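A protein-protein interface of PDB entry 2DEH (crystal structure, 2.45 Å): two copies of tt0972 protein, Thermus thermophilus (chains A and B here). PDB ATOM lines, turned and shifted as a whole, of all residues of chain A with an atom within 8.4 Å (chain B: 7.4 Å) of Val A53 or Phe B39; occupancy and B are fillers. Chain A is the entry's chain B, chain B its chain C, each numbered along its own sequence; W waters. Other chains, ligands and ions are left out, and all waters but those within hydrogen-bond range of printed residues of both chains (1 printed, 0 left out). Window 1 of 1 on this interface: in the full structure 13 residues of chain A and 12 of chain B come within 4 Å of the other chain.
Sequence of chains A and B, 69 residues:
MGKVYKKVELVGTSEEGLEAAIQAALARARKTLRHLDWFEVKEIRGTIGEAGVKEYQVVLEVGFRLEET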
ATOM      1  N   SER A  14      -4.447   6.341   8.149  1.00  0.00           N
ATOM      2  CA  SER A  14      -3.623   5.481   8.988  1.00  0.00           C
ATOM      3  C   SER A  14      -2.187   5.988   9.023  1.00  0.00           C
ATOM      4  O   SER A  14      -1.672   6.511   8.031  1.00  0.00           O
ATOM      5  CB  SER A  14      -3.644   4.047   8.451  1.00  0.00           C
ATOM      6  OG  SER A  14      -2.748   3.212   9.175  1.00  0.00           O
ATOM      7  N   GLU A  15      -1.542   5.829  10.174  1.00  0.00           N
ATOM      8  CA  GLU A  15      -0.158   6.261  10.331  1.00  0.00           C
ATOM      9  C   GLU A  15       0.814   5.164   9.890  1.00  0.00           C
ATOM     10  O   GLU A  15       2.017   5.405   9.752  1.00  0.00           O
ATOM     11  CB  GLU A  15       0.100   6.614  11.794  1.00  0.00           C
ATOM     12  CG  GLU A  15      -0.845   7.690  12.336  1.00  0.00           C
ATOM     13  CD  GLU A  15      -0.498   8.113  13.759  1.00  0.00           C
ATOM     14  OE1 GLU A  15       0.710   8.110  14.101  1.00  0.00           O
ATOM     15  OE2 GLU A  15      -1.425   8.453  14.529  1.00  0.00           O
ATOM     16  N   GLU A  16       0.275   3.973   9.641  1.00  0.00           N
ATOM     17  CA  GLU A  16       1.075   2.816   9.265  1.00  0.00           C
ATOM     18  C   GLU A  16       1.395   2.668   7.784  1.00  0.00           C
ATOM     19  O   GLU A  16       2.551   2.426   7.410  1.00  0.00           O
ATOM     20  CB  GLU A  16       0.386   1.550   9.772  1.00  0.00           C
ATOM     21  CG  GLU A  16       0.354   1.487  11.298  1.00  0.00           C
ATOM     22  CD  GLU A  16      -0.512   0.356  11.834  1.00  0.00           C
ATOM     23  OE1 GLU A  16      -0.666  -0.669  11.128  1.00  0.00           O
ATOM     24  OE2 GLU A  16      -1.035   0.495  12.966  1.00  0.00           O
ATOM     25  N   GLY A  17       0.381   2.803   6.937  1.00  0.00           N
ATOM     26  CA  GLY A  17       0.619   2.654   5.516  1.00  0.00           C
ATOM     27  C   GLY A  17      -0.636   2.674   4.672  1.00  0.00           C
ATOM     28  O   GLY A  17      -1.750   2.823   5.181  1.00  0.00           O
ATOM     29  N   LEU A  18      -0.438   2.513   3.367  1.00  0.00           N
ATOM     30  CA  LEU A  18      -1.540   2.538   2.414  1.00  0.00           C
ATOM     31  C   LEU A  18      -2.551   1.416   2.679  1.00  0.00           C
ATOM     32  O   LEU A  18      -3.753   1.680   2.831  1.00  0.00           O
ATOM     33  CB  LEU A  18      -0.990   2.462   0.983  1.00  0.00           C
ATOM     34  CG  LEU A  18       0.049   3.562   0.687  1.00  0.00           C
ATOM     35  CD1 LEU A  18       0.593   3.399  -0.712  1.00  0.00           C
ATOM     36  CD2 LEU A  18      -0.562   4.952   0.857  1.00  0.00           C
ATOM     37  N   GLU A  43      -7.576   8.490  -4.814  1.00  0.00           N
ATOM     38  CA  GLU A  43      -6.436   9.346  -4.514  1.00  0.00           C
ATOM     39  C   GLU A  43      -5.672   8.773  -3.363  1.00  0.00           C
ATOM     40  O   GLU A  43      -6.192   7.990  -2.569  1.00  0.00           O
ATOM     41  CB  GLU A  43      -6.828  10.763  -4.086  1.00  0.00           C
ATOM     42  CG  GLU A  43      -7.970  11.383  -4.804  1.00  0.00           C
ATOM     43  CD  GLU A  43      -8.402  12.680  -4.139  1.00  0.00           C
ATOM     44  OE1 GLU A  43      -9.611  13.028  -4.233  1.00  0.00           O
ATOM     45  OE2 GLU A  43      -7.518  13.341  -3.530  1.00  0.00           O
ATOM     46  N   ILE A  44      -4.419   9.188  -3.298  1.00  0.00           N
ATOM     47  CA  ILE A  44      -3.541   8.837  -2.217  1.00  0.00           C
ATOM     48  C   ILE A  44      -2.871  10.148  -1.883  1.00  0.00           C
ATOM     49  O   ILE A  44      -2.281  10.774  -2.742  1.00  0.00           O
ATOM     50  CB  ILE A  44      -2.494   7.774  -2.638  1.00  0.00           C
ATOM     51  CG1 ILE A  44      -3.153   6.388  -2.696  1.00  0.00           C
ATOM     52  CG2 ILE A  44      -1.292   7.783  -1.659  1.00  0.00           C
ATOM     53  CD1 ILE A  44      -2.288   5.351  -3.377  1.00  0.00           C
ATOM     54  N   ARG A  45      -3.048  10.607  -0.655  1.00  0.00           N
ATOM     55  CA  ARG A  45      -2.383  11.824  -0.190  1.00  0.00           C
ATOM     56  C   ARG A  45      -2.032  11.585   1.295  1.00  0.00           C
ATOM     57  O   ARG A  45      -2.198  10.476   1.830  1.00  0.00           O
ATOM     58  CB  ARG A  45      -3.285  13.076  -0.315  1.00  0.00           C
ATOM     59  CG  ARG A  45      -4.638  12.880  -0.979  1.00  0.00           C
ATOM     60  CD  ARG A  45      -5.662  14.003  -0.634  1.00  0.00           C
ATOM     61  NE  ARG A  45      -5.465  15.285  -1.329  1.00  0.00           N
ATOM     62  CZ  ARG A  45      -5.132  16.438  -0.737  1.00  0.00           C
ATOM     63  NH1 ARG A  45      -4.941  16.491   0.586  1.00  0.00           N
ATOM     64  NH2 ARG A  45      -5.011  17.547  -1.466  1.00  0.00           N
ATOM     65  N   GLY A  46      -1.562  12.628   1.967  1.00  0.00           N
ATOM     66  CA  GLY A  46      -1.250  12.479   3.366  1.00  0.00           C
ATOM     67  C   GLY A  46      -0.718  13.752   3.959  1.00  0.00           C
ATOM     68  O   GLY A  46      -0.472  14.731   3.248  1.00  0.00           O
ATOM     69  N   THR A  47      -0.550  13.739   5.276  1.00  0.00           N
ATOM     70  CA  THR A  47      -0.017  14.884   5.999  1.00  0.00           C
ATOM     71  C   THR A  47       1.429  14.604   6.351  1.00  0.00           C
ATOM     72  O   THR A  47       1.833  13.444   6.437  1.00  0.00           O
ATOM     73  CB  THR A  47      -0.770  15.119   7.281  1.00  0.00           C
ATOM     74  OG1 THR A  47      -0.871  13.877   7.987  1.00  0.00           O
ATOM     75  CG2 THR A  47      -2.153  15.674   6.988  1.00  0.00           C
ATOM     76  N   ILE A  48       2.189  15.675   6.561  1.00  0.00           N
ATOM     77  CA  ILE A  48       3.604  15.582   6.873  1.00  0.00           C
ATOM     78  C   ILE A  48       3.913  16.031   8.298  1.00  0.00           C
ATOM     79  O   ILE A  48       3.456  17.088   8.751  1.00  0.00           O
ATOM     80  CB  ILE A  48       4.412  16.432   5.878  1.00  0.00           C
ATOM     81  CG1 ILE A  48       4.069  15.991   4.447  1.00  0.00           C
ATOM     82  CG2 ILE A  48       5.892  16.288   6.147  1.00  0.00           C
ATOM     83  CD1 ILE A  48       4.837  16.699   3.366  1.00  0.00           C
ATOM     84  N   GLY A  49       4.694  15.202   8.988  1.00  0.00           N
ATOM     85  CA  GLY A  49       5.089  15.476  10.356  1.00  0.00           C
ATOM     86  C   GLY A  49       6.593  15.564  10.456  1.00  0.00           C
ATOM     87  O   GLY A  49       7.273  15.624   9.433  1.00  0.00           O
ATOM     88  N   GLU A  50       7.113  15.609  11.680  1.00  0.00           N
ATOM     89  CA  GLU A  50       8.553  15.744  11.893  1.00  0.00           C
ATOM     90  C   GLU A  50       9.346  14.522  11.427  1.00  0.00           C
ATOM     91  O   GLU A  50      10.530  14.630  11.094  1.00  0.00           O
ATOM     92  CB  GLU A  50       8.821  16.014  13.376  1.00  0.00           C
ATOM     93  CG  GLU A  50       8.130  17.283  13.892  1.00  0.00           C
ATOM     94  CD  GLU A  50       9.000  18.533  13.736  1.00  0.00           C
ATOM     95  OE1 GLU A  50      10.010  18.454  13.002  1.00  0.00           O
ATOM     96  OE2 GLU A  50       8.680  19.589  14.346  1.00  0.00           O
ATOM     97  N   ALA A  51       8.693  13.362  11.416  1.00  0.00           N
ATOM     98  CA  ALA A  51       9.331  12.109  11.005  1.00  0.00           C
ATOM     99  C   ALA A  51       8.982  11.736   9.554  1.00  0.00           C
ATOM    100  O   ALA A  51       9.250  10.621   9.087  1.00  0.00           O
ATOM    101  CB  ALA A  51       8.921  10.976  11.970  1.00  0.00           C
ATOM    102  N   GLY A  52       8.406  12.695   8.837  1.00  0.00           N
ATOM    103  CA  GLY A  52       8.022  12.456   7.456  1.00  0.00           C
ATOM    104  C   GLY A  52       6.515  12.325   7.383  1.00  0.00           C
ATOM    105  O   GLY A  52       5.801  13.237   7.816  1.00  0.00           O
ATOM    106  N   VAL A  53       6.024  11.190   6.881  1.00  0.00           N
ATOM    107  CA  VAL A  53       4.585  10.987   6.789  1.00  0.00           C
ATOM    108  C   VAL A  53       3.991  10.928   8.180  1.00  0.00           C
ATOM    109  O   VAL A  53       4.491  10.197   9.031  1.00  0.00           O
ATOM    110  CB  VAL A  53       4.210   9.669   6.055  1.00  0.00           C
ATOM    111  CG1 VAL A  53       2.707   9.489   6.069  1.00  0.00           C
ATOM    112  CG2 VAL A  53       4.698   9.705   4.621  1.00  0.00           C
ATOM    113  N   LYS A  54       2.948  11.725   8.410  1.00  0.00           N
ATOM    114  CA  LYS A  54       2.244  11.730   9.685  1.00  0.00           C
ATOM    115  C   LYS A  54       1.164  10.710   9.497  1.00  0.00           C
ATOM    116  O   LYS A  54       1.181   9.661  10.104  1.00  0.00           O
ATOM    117  CB  LYS A  54       1.633  13.107   9.968  1.00  0.00           C
ATOM    118  CG  LYS A  54       1.110  13.293  11.402  1.00  0.00           C
ATOM    119  CD  LYS A  54       0.290  14.566  11.539  1.00  0.00           C
ATOM    120  CE  LYS A  54       1.078  15.811  11.115  1.00  0.00           C
ATOM    121  NZ  LYS A  54       0.205  17.022  11.130  1.00  0.00           N
ATOM    122  N   GLU A  55       0.266  10.994   8.568  1.00  0.00           N
ATOM    123  CA  GLU A  55      -0.821  10.073   8.293  1.00  0.00           C
ATOM    124  C   GLU A  55      -1.089   9.879   6.801  1.00  0.00           C
ATOM    125  O   GLU A  55      -1.040  10.839   6.027  1.00  0.00           O
ATOM    126  CB  GLU A  55      -2.079  10.547   9.035  1.00  0.00           C
ATOM    127  CG  GLU A  55      -3.355  10.598   8.232  1.00  0.00           C
ATOM    128  CD  GLU A  55      -4.472  11.266   9.021  1.00  0.00           C
ATOM    129  OE1 GLU A  55      -4.600  10.940  10.225  1.00  0.00           O
ATOM    130  OE2 GLU A  55      -5.217  12.100   8.447  1.00  0.00           O
ATOM    131  N   TYR A  56      -1.323   8.633   6.396  1.00  0.00           N
ATOM    132  CA  TYR A  56      -1.624   8.334   5.004  1.00  0.00           C
ATOM    133  C   TYR A  56      -3.131   8.491   4.849  1.00  0.00           C
ATOM    134  O   TYR A  56      -3.893   8.113   5.732  1.00  0.00           O
ATOM    135  CB  TYR A  56      -1.221   6.897   4.656  1.00  0.00           C
ATOM    136  CG  TYR A  56       0.272   6.673   4.608  1.00  0.00           C
ATOM    137  CD1 TYR A  56       1.025   7.094   3.512  1.00  0.00           C
ATOM    138  CD2 TYR A  56       0.941   6.059   5.672  1.00  0.00           C
ATOM    139  CE1 TYR A  56       2.431   6.910   3.475  1.00  0.00           C
ATOM    140  CE2 TYR A  56       2.344   5.868   5.651  1.00  0.00           C
ATOM    141  CZ  TYR A  56       3.086   6.298   4.554  1.00  0.00           C
ATOM    142  OH  TYR A  56       4.468   6.153   4.563  1.00  0.00           O
ATOM    143  N   GLN A  57      -3.553   9.053   3.725  1.00  0.00           N
ATOM    144  CA  GLN A  57      -4.970   9.257   3.466  1.00  0.00           C
ATOM    145  C   GLN A  57      -5.312   8.663   2.097  1.00  0.00           C
ATOM    146  O   GLN A  57      -4.788   9.113   1.077  1.00  0.00           O
ATOM    147  CB  GLN A  57      -5.285  10.757   3.500  1.00  0.00           C
ATOM    148  CG  GLN A  57      -4.967  11.414   4.840  1.00  0.00           C
ATOM    149  CD  GLN A  57      -5.121  12.933   4.831  1.00  0.00           C
ATOM    150  OE1 GLN A  57      -5.299  13.556   5.886  1.00  0.00           O
ATOM    151  NE2 GLN A  57      -5.033  13.539   3.643  1.00  0.00           N
ATOM    152  N   LYS B   7       3.669  24.307  -3.862  1.00  0.00           N
ATOM    153  CA  LYS B   7       3.740  22.879  -4.086  1.00  0.00           C
ATOM    154  C   LYS B   7       4.908  22.598  -5.014  1.00  0.00           C
ATOM    155  O   LYS B   7       5.123  23.311  -6.003  1.00  0.00           O
ATOM    156  CB  LYS B   7       2.428  22.369  -4.694  1.00  0.00           C
ATOM    157  CG  LYS B   7       1.222  22.507  -3.783  1.00  0.00           C
ATOM    158  CD  LYS B   7      -0.075  22.246  -4.548  1.00  0.00           C
ATOM    159  CE  LYS B   7      -0.221  20.789  -4.985  1.00  0.00           C
ATOM    160  NZ  LYS B   7      -1.424  20.605  -5.837  1.00  0.00           N
ATOM    161  N   GLU B  19       5.499   3.043   0.358  1.00  0.00           N
ATOM    162  CA  GLU B  19       5.653   3.913   1.520  1.00  0.00           C
ATOM    163  C   GLU B  19       7.086   4.417   1.656  1.00  0.00           C
ATOM    164  O   GLU B  19       7.315   5.590   1.974  1.00  0.00           O
ATOM    165  CB  GLU B  19       5.229   3.192   2.803  1.00  0.00           C
ATOM    166  CG  GLU B  19       3.729   2.980   2.927  1.00  0.00           C
ATOM    167  CD  GLU B  19       3.279   1.660   2.319  1.00  0.00           C
ATOM    168  OE1 GLU B  19       4.108   1.018   1.629  1.00  0.00           O
ATOM    169  OE2 GLU B  19       2.099   1.262   2.529  1.00  0.00           O
ATOM    170  N   ILE B  22       7.805   7.157  -0.836  1.00  0.00           N
ATOM    171  CA  ILE B  22       7.211   8.416  -0.390  1.00  0.00           C
ATOM    172  C   ILE B  22       8.091   9.056   0.693  1.00  0.00           C
ATOM    173  O   ILE B  22       8.419  10.237   0.611  1.00  0.00           O
ATOM    174  CB  ILE B  22       5.790   8.186   0.167  1.00  0.00           C
ATOM    175  CG1 ILE B  22       4.846   7.817  -0.988  1.00  0.00           C
ATOM    176  CG2 ILE B  22       5.317   9.415   0.925  1.00  0.00           C
ATOM    177  CD1 ILE B  22       3.453   7.426  -0.553  1.00  0.00           C
ATOM    178  N   GLN B  23       8.456   8.269   1.705  1.00  0.00           N
ATOM    179  CA  GLN B  23       9.317   8.731   2.802  1.00  0.00           C
ATOM    180  C   GLN B  23      10.653   9.282   2.274  1.00  0.00           C
ATOM    181  O   GLN B  23      11.120  10.335   2.716  1.00  0.00           O
ATOM    182  CB  GLN B  23       9.581   7.575   3.779  1.00  0.00           C
ATOM    183  CG  GLN B  23       8.347   7.114   4.521  1.00  0.00           C
ATOM    184  CD  GLN B  23       8.009   8.031   5.666  1.00  0.00           C
ATOM    185  OE1 GLN B  23       8.397   9.205   5.676  1.00  0.00           O
ATOM    186  NE2 GLN B  23       7.274   7.505   6.646  1.00  0.00           N
ATOM    187  N   LEU B  26      10.114  12.684   1.084  1.00  0.00           N
ATOM    188  CA  LEU B  26       9.813  13.594   2.185  1.00  0.00           C
ATOM    189  C   LEU B  26      11.083  13.900   2.977  1.00  0.00           C
ATOM    190  O   LEU B  26      11.315  15.050   3.388  1.00  0.00           O
ATOM    191  CB  LEU B  26       8.736  13.001   3.100  1.00  0.00           C
ATOM    192  CG  LEU B  26       7.346  12.889   2.454  1.00  0.00           C
ATOM    193  CD1 LEU B  26       6.344  12.490   3.494  1.00  0.00           C
ATOM    194  CD2 LEU B  26       6.920  14.221   1.838  1.00  0.00           C
ATOM    195  N   ALA B  27      11.914  12.875   3.170  1.00  0.00           N
ATOM    196  CA  ALA B  27      13.170  13.053   3.890  1.00  0.00           C
ATOM    197  C   ALA B  27      13.990  14.126   3.183  1.00  0.00           C
ATOM    198  O   ALA B  27      14.387  15.122   3.788  1.00  0.00           O
ATOM    199  CB  ALA B  27      13.953  11.737   3.937  1.00  0.00           C
ATOM    200  N   LEU B  36       6.672  21.843   5.890  1.00  0.00           N
ATOM    201  CA  LEU B  36       6.044  20.853   5.039  1.00  0.00           C
ATOM    202  C   LEU B  36       4.712  20.482   5.669  1.00  0.00           C
ATOM    203  O   LEU B  36       4.676  20.104   6.837  1.00  0.00           O
ATOM    204  CB  LEU B  36       6.940  19.620   4.906  1.00  0.00           C
ATOM    205  CG  LEU B  36       8.250  19.880   4.146  1.00  0.00           C
ATOM    206  CD1 LEU B  36       9.121  18.630   4.174  1.00  0.00           C
ATOM    207  CD2 LEU B  36       7.950  20.296   2.704  1.00  0.00           C
ATOM    208  N   ASP B  37       3.621  20.606   4.907  1.00  0.00           N
ATOM    209  CA  ASP B  37       2.297  20.269   5.439  1.00  0.00           C
ATOM    210  C   ASP B  37       1.636  19.027   4.852  1.00  0.00           C
ATOM    211  O   ASP B  37       1.219  18.143   5.609  1.00  0.00           O
ATOM    212  CB  ASP B  37       1.316  21.451   5.314  1.00  0.00           C
ATOM    213  CG  ASP B  37       1.697  22.629   6.211  1.00  0.00           C
ATOM    214  OD1 ASP B  37       2.131  22.384   7.361  1.00  0.00           O
ATOM    215  OD2 ASP B  37       1.561  23.799   5.779  1.00  0.00           O
ATOM    216  N   TRP B  38       1.517  18.952   3.523  1.00  0.00           N
ATOM    217  CA  TRP B  38       0.860  17.793   2.916  1.00  0.00           C
ATOM    218  C   TRP B  38       1.457  17.344   1.598  1.00  0.00           C
ATOM    219  O   TRP B  38       2.207  18.072   0.947  1.00  0.00           O
ATOM    220  CB  TRP B  38      -0.641  18.071   2.713  1.00  0.00           C
ATOM    221  CG  TRP B  38      -0.966  18.806   1.434  1.00  0.00           C
ATOM    222  CD1 TRP B  38      -1.442  18.257   0.274  1.00  0.00           C
ATOM    223  CD2 TRP B  38      -0.790  20.209   1.168  1.00  0.00           C
ATOM    224  NE1 TRP B  38      -1.582  19.227  -0.689  1.00  0.00           N
ATOM    225  CE2 TRP B  38      -1.205  20.436  -0.168  1.00  0.00           C
ATOM    226  CE3 TRP B  38      -0.350  21.303   1.936  1.00  0.00           C
ATOM    227  CZ2 TRP B  38      -1.156  21.704  -0.773  1.00  0.00           C
ATOM    228  CZ3 TRP B  38      -0.301  22.573   1.336  1.00  0.00           C
ATOM    229  CH2 TRP B  38      -0.720  22.761  -0.004  1.00  0.00           C
ATOM    230  N   PHE B  39       1.125  16.115   1.224  1.00  0.00           N
ATOM    231  CA  PHE B  39       1.587  15.564  -0.037  1.00  0.00           C
ATOM    232  C   PHE B  39       0.413  14.901  -0.767  1.00  0.00           C
ATOM    233  O   PHE B  39      -0.606  14.540  -0.165  1.00  0.00           O
ATOM    234  CB  PHE B  39       2.748  14.583   0.192  1.00  0.00           C
ATOM    235  CG  PHE B  39       2.351  13.293   0.845  1.00  0.00           C
ATOM    236  CD1 PHE B  39       1.814  12.246   0.095  1.00  0.00           C
ATOM    237  CD2 PHE B  39       2.529  13.109   2.219  1.00  0.00           C
ATOM    238  CE1 PHE B  39       1.462  11.041   0.710  1.00  0.00           C
ATOM    239  CE2 PHE B  39       2.177  11.899   2.838  1.00  0.00           C
ATOM    240  CZ  PHE B  39       1.645  10.870   2.084  1.00  0.00           C
ATOM    241  N   GLU B  40       0.564  14.789  -2.073  1.00  0.00           N
ATOM    242  CA  GLU B  40      -0.440  14.199  -2.935  1.00  0.00           C
ATOM    243  C   GLU B  40       0.320  13.321  -3.909  1.00  0.00           C
ATOM    244  O   GLU B  40       1.272  13.775  -4.555  1.00  0.00           O
ATOM    245  CB  GLU B  40      -1.176  15.298  -3.716  1.00  0.00           C
ATOM    246  CG  GLU B  40      -1.828  16.394  -2.859  1.00  0.00           C
ATOM    247  CD  GLU B  40      -2.198  17.639  -3.656  1.00  0.00           C
ATOM    248  OE1 GLU B  40      -2.073  17.623  -4.894  1.00  0.00           O
ATOM    249  OE2 GLU B  40      -2.607  18.647  -3.052  1.00  0.00           O
ATOM    250  N   VAL B  41      -0.078  12.063  -3.997  1.00  0.00           N
ATOM    251  CA  VAL B  41       0.548  11.155  -4.933  1.00  0.00           C
ATOM    252  C   VAL B  41      -0.064  11.369  -6.326  1.00  0.00           C
ATOM    253  O   VAL B  41      -1.284  11.355  -6.493  1.00  0.00           O
ATOM    254  CB  VAL B  41       0.327   9.699  -4.522  1.00  0.00           C
ATOM    255  CG1 VAL B  41       0.781   8.773  -5.642  1.00  0.00           C
ATOM    256  CG2 VAL B  41       1.099   9.400  -3.237  1.00  0.00           C
ATOM    257  N   LYS B  42       0.781  11.579  -7.324  1.00  0.00           N
ATOM    258  CA  LYS B  42       0.305  11.778  -8.682  1.00  0.00           C
ATOM    259  C   LYS B  42       0.472  10.514  -9.529  1.00  0.00           C
ATOM    260  O   LYS B  42      -0.456  10.105 -10.216  1.00  0.00           O
ATOM    261  CB  LYS B  42       1.054  12.950  -9.314  1.00  0.00           C
ATOM    262  CG  LYS B  42       0.887  14.215  -8.521  1.00  0.00           C
ATOM    263  CD  LYS B  42      -0.570  14.659  -8.586  1.00  0.00           C
ATOM    264  CE  LYS B  42      -1.003  15.425  -7.336  1.00  0.00           C
ATOM    265  NZ  LYS B  42      -1.925  16.550  -7.696  1.00  0.00           N
ATOM    266  N   VAL B  58       7.545   6.980  -6.973  1.00  0.00           N
ATOM    267  CA  VAL B  58       6.291   7.634  -6.691  1.00  0.00           C
ATOM    268  C   VAL B  58       6.414   9.132  -6.909  1.00  0.00           C
ATOM    269  O   VAL B  58       7.184   9.830  -6.226  1.00  0.00           O
ATOM    270  CB  VAL B  58       5.833   7.367  -5.244  1.00  0.00           C
ATOM    271  CG1 VAL B  58       4.550   8.134  -4.948  1.00  0.00           C
ATOM    272  CG2 VAL B  58       5.579   5.884  -5.050  1.00  0.00           C
ATOM    273  N   LEU B  60       5.031  12.685  -6.556  1.00  0.00           N
ATOM    274  CA  LEU B  60       4.131  13.302  -5.605  1.00  0.00           C
ATOM    275  C   LEU B  60       4.392  14.773  -5.460  1.00  0.00           C
ATOM    276  O   LEU B  60       5.475  15.276  -5.788  1.00  0.00           O
ATOM    277  CB  LEU B  60       4.245  12.615  -4.242  1.00  0.00           C
ATOM    278  CG  LEU B  60       5.625  12.515  -3.580  1.00  0.00           C
ATOM    279  CD1 LEU B  60       6.090  13.886  -3.127  1.00  0.00           C
ATOM    280  CD2 LEU B  60       5.524  11.591  -2.374  1.00  0.00           C
ATOM    281  N   GLU B  61       3.372  15.475  -4.993  1.00  0.00           N
ATOM    282  CA  GLU B  61       3.515  16.890  -4.804  1.00  0.00           C
ATOM    283  C   GLU B  61       3.548  17.111  -3.315  1.00  0.00           C
ATOM    284  O   GLU B  61       2.816  16.467  -2.549  1.00  0.00           O
ATOM    285  CB  GLU B  61       2.367  17.639  -5.473  1.00  0.00           C
ATOM    286  CG  GLU B  61       2.387  17.468  -6.977  1.00  0.00           C
ATOM    287  CD  GLU B  61       1.358  18.316  -7.690  1.00  0.00           C
ATOM    288  OE1 GLU B  61       0.198  18.345  -7.220  1.00  0.00           O
ATOM    289  OE2 GLU B  61       1.706  18.938  -8.725  1.00  0.00           O
ATOM    290  N   VAL B  62       4.439  18.006  -2.915  1.00  0.00           N
ATOM    291  CA  VAL B  62       4.622  18.343  -1.525  1.00  0.00           C
ATOM    292  C   VAL B  62       4.233  19.784  -1.357  1.00  0.00           C
ATOM    293  O   VAL B  62       4.754  20.654  -2.051  1.00  0.00           O
ATOM    294  CB  VAL B  62       6.078  18.173  -1.114  1.00  0.00           C
ATOM    295  CG1 VAL B  62       6.274  18.668   0.306  1.00  0.00           C
ATOM    296  CG2 VAL B  62       6.464  16.720  -1.230  1.00  0.00           C
ATOM    297  N   GLY B  63       3.298  20.025  -0.443  1.00  0.00           N
ATOM    298  CA  GLY B  63       2.837  21.371  -0.185  1.00  0.00           C
ATOM    299  C   GLY B  63       3.362  21.853   1.148  1.00  0.00           C
ATOM    300  O   GLY B  63       3.399  21.119   2.141  1.00  0.00           O
HETATM  301  O   HOH W   1      -3.286   9.583  -6.021  1.00  0.00           O
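No position is printed for both chains. Of the 26 pairs that touch across the chains among the printed residues, none has its exchanged pair printed and touching as well.
Val A53 touches just these residues of chain B: Ile B22 (3.8 Å), Gln B23 (3.3 Å), Leu B26 (3.4 Å) and Phe B39 (3.8 Å). Phe B39 touches five residues of chain A. Of the printed residues of chain B, Ile A44 touches Glu B40 (3.8 Å) and Val B41 (2.8 Å). Of the printed residues of chain A, Trp B38 touches Arg A45 (3.9 Å), Gly A46 (3.4 Å) and Ile A48 (3.8 Å). Of the printed residues of chain A, Val B62 touches Ile A48. Ala B27 touches none of the printed residues of chain A. Gly B63 touches none of the printed residues of chain A. The nearest printed residue of chain B that does not touch Leu A18 is Ile B22 (4.9 Å).
Among the printed residues, pairs that only touch across the chains: Gly A17 with Glu B19, Ile A44 with Glu B40, Arg A45 with Trp B38, Arg A45 with Phe B39, Gly A46 with Trp B38, Thr A47 with Asp B37, Thr A47 with Phe B39, Ile A48 with Leu B26, Ile A48 with Leu B36, Ile A48 with Trp B38, Ile A48 with Phe B39, Ile A48 with Val B62, Ala A51 with Gln B23, Gly A52 with Gln B23, Gly A52 with Leu B26, Val A53 with Ile B22, Val A53 with Leu B26, Val A53 with Phe B39, Tyr A56 with Glu B19 and Tyr A56 with Gln B23.
Water W1 bridges the backbone carbonyl oxygen (O) of Val B41 (2.7 Å) and the backbone NH (N) of Ile A44 (3.0 Å).
Of the 20 printed residues of chain A, 11 touch a printed residue of chain B. Printed residues of chain A that touch a printed residue of chain B: Gly A17, Leu A18, Ile A44, Arg A45, Gly A46, Thr A47, Ile A48, Ala A51, Gly A52, Val A53 and Tyr A56. Printed residues of chain B that touch a printed residue of chain A: Glu B19, Ile B22, Gln B23, Leu B26, Leu B36, Asp B37, Trp B38, Phe B39, Glu B40, Val B41 and Val B62. Hydrophobic or aromatic side chains of chain B that line the printed part of chain A: Ile B22, Leu B26, Leu B36, Trp B38, Phe B39, Val B41 and Val B62. Among the printed residues, Asp or Glu carboxylates within 4 Å of a Lys or Arg side-chain nitrogen of the other chain: Arg A45 with Glu B40.
O of Ser A14 sits at hydrogen-bond distance from N of Tyr A56, at 2.7 Å. The backbone carbonyl oxygen (O) of Glu A55 lies within hydrogen-bond range of the backbone NH (N) of Thr A47 (3.0 Å). The side-chain amino group (NZ) of Lys B7 is in salt-bridge range of the side-chain carboxylate (OE1) of Glu B40, 3.2 Å away. OE2 of Glu B40 lies within hydrogen-bond range of NE1 of Trp B38 (2.6 Å). The backbone carbonyl oxygen of Trp B38 lies within hydrogen-bond range of the backbone NH of Gly B63 (2.6 Å). OE1 of Glu B40 is in salt-bridge range of NZ of Lys B42 (3.0 Å).
The backbone NH (N) of Leu A18 is in hydrogen-bond range of the side-chain carboxylate (OE2) of Glu B19, at 3.0 Å. The backbone NH (N) of Val B41 sits at hydrogen-bond distance from the backbone carbonyl oxygen (O) of Ile A44 (2.8 Å). OE2 of Glu B40 is in salt-bridge range of NH2 of Arg A45, at 3.1 Å. The backbone NH of Phe B39 sits at hydrogen-bond distance from the backbone carbonyl oxygen of Gly A46. The backbone NH (N) of Ile A48 sits at hydrogen-bond distance from the backbone carbonyl oxygen (O) of Asp B37 (2.8 Å). N of Val A53 sits at hydrogen-bond distance from OE1 of Gln B23 (3.3 Å).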
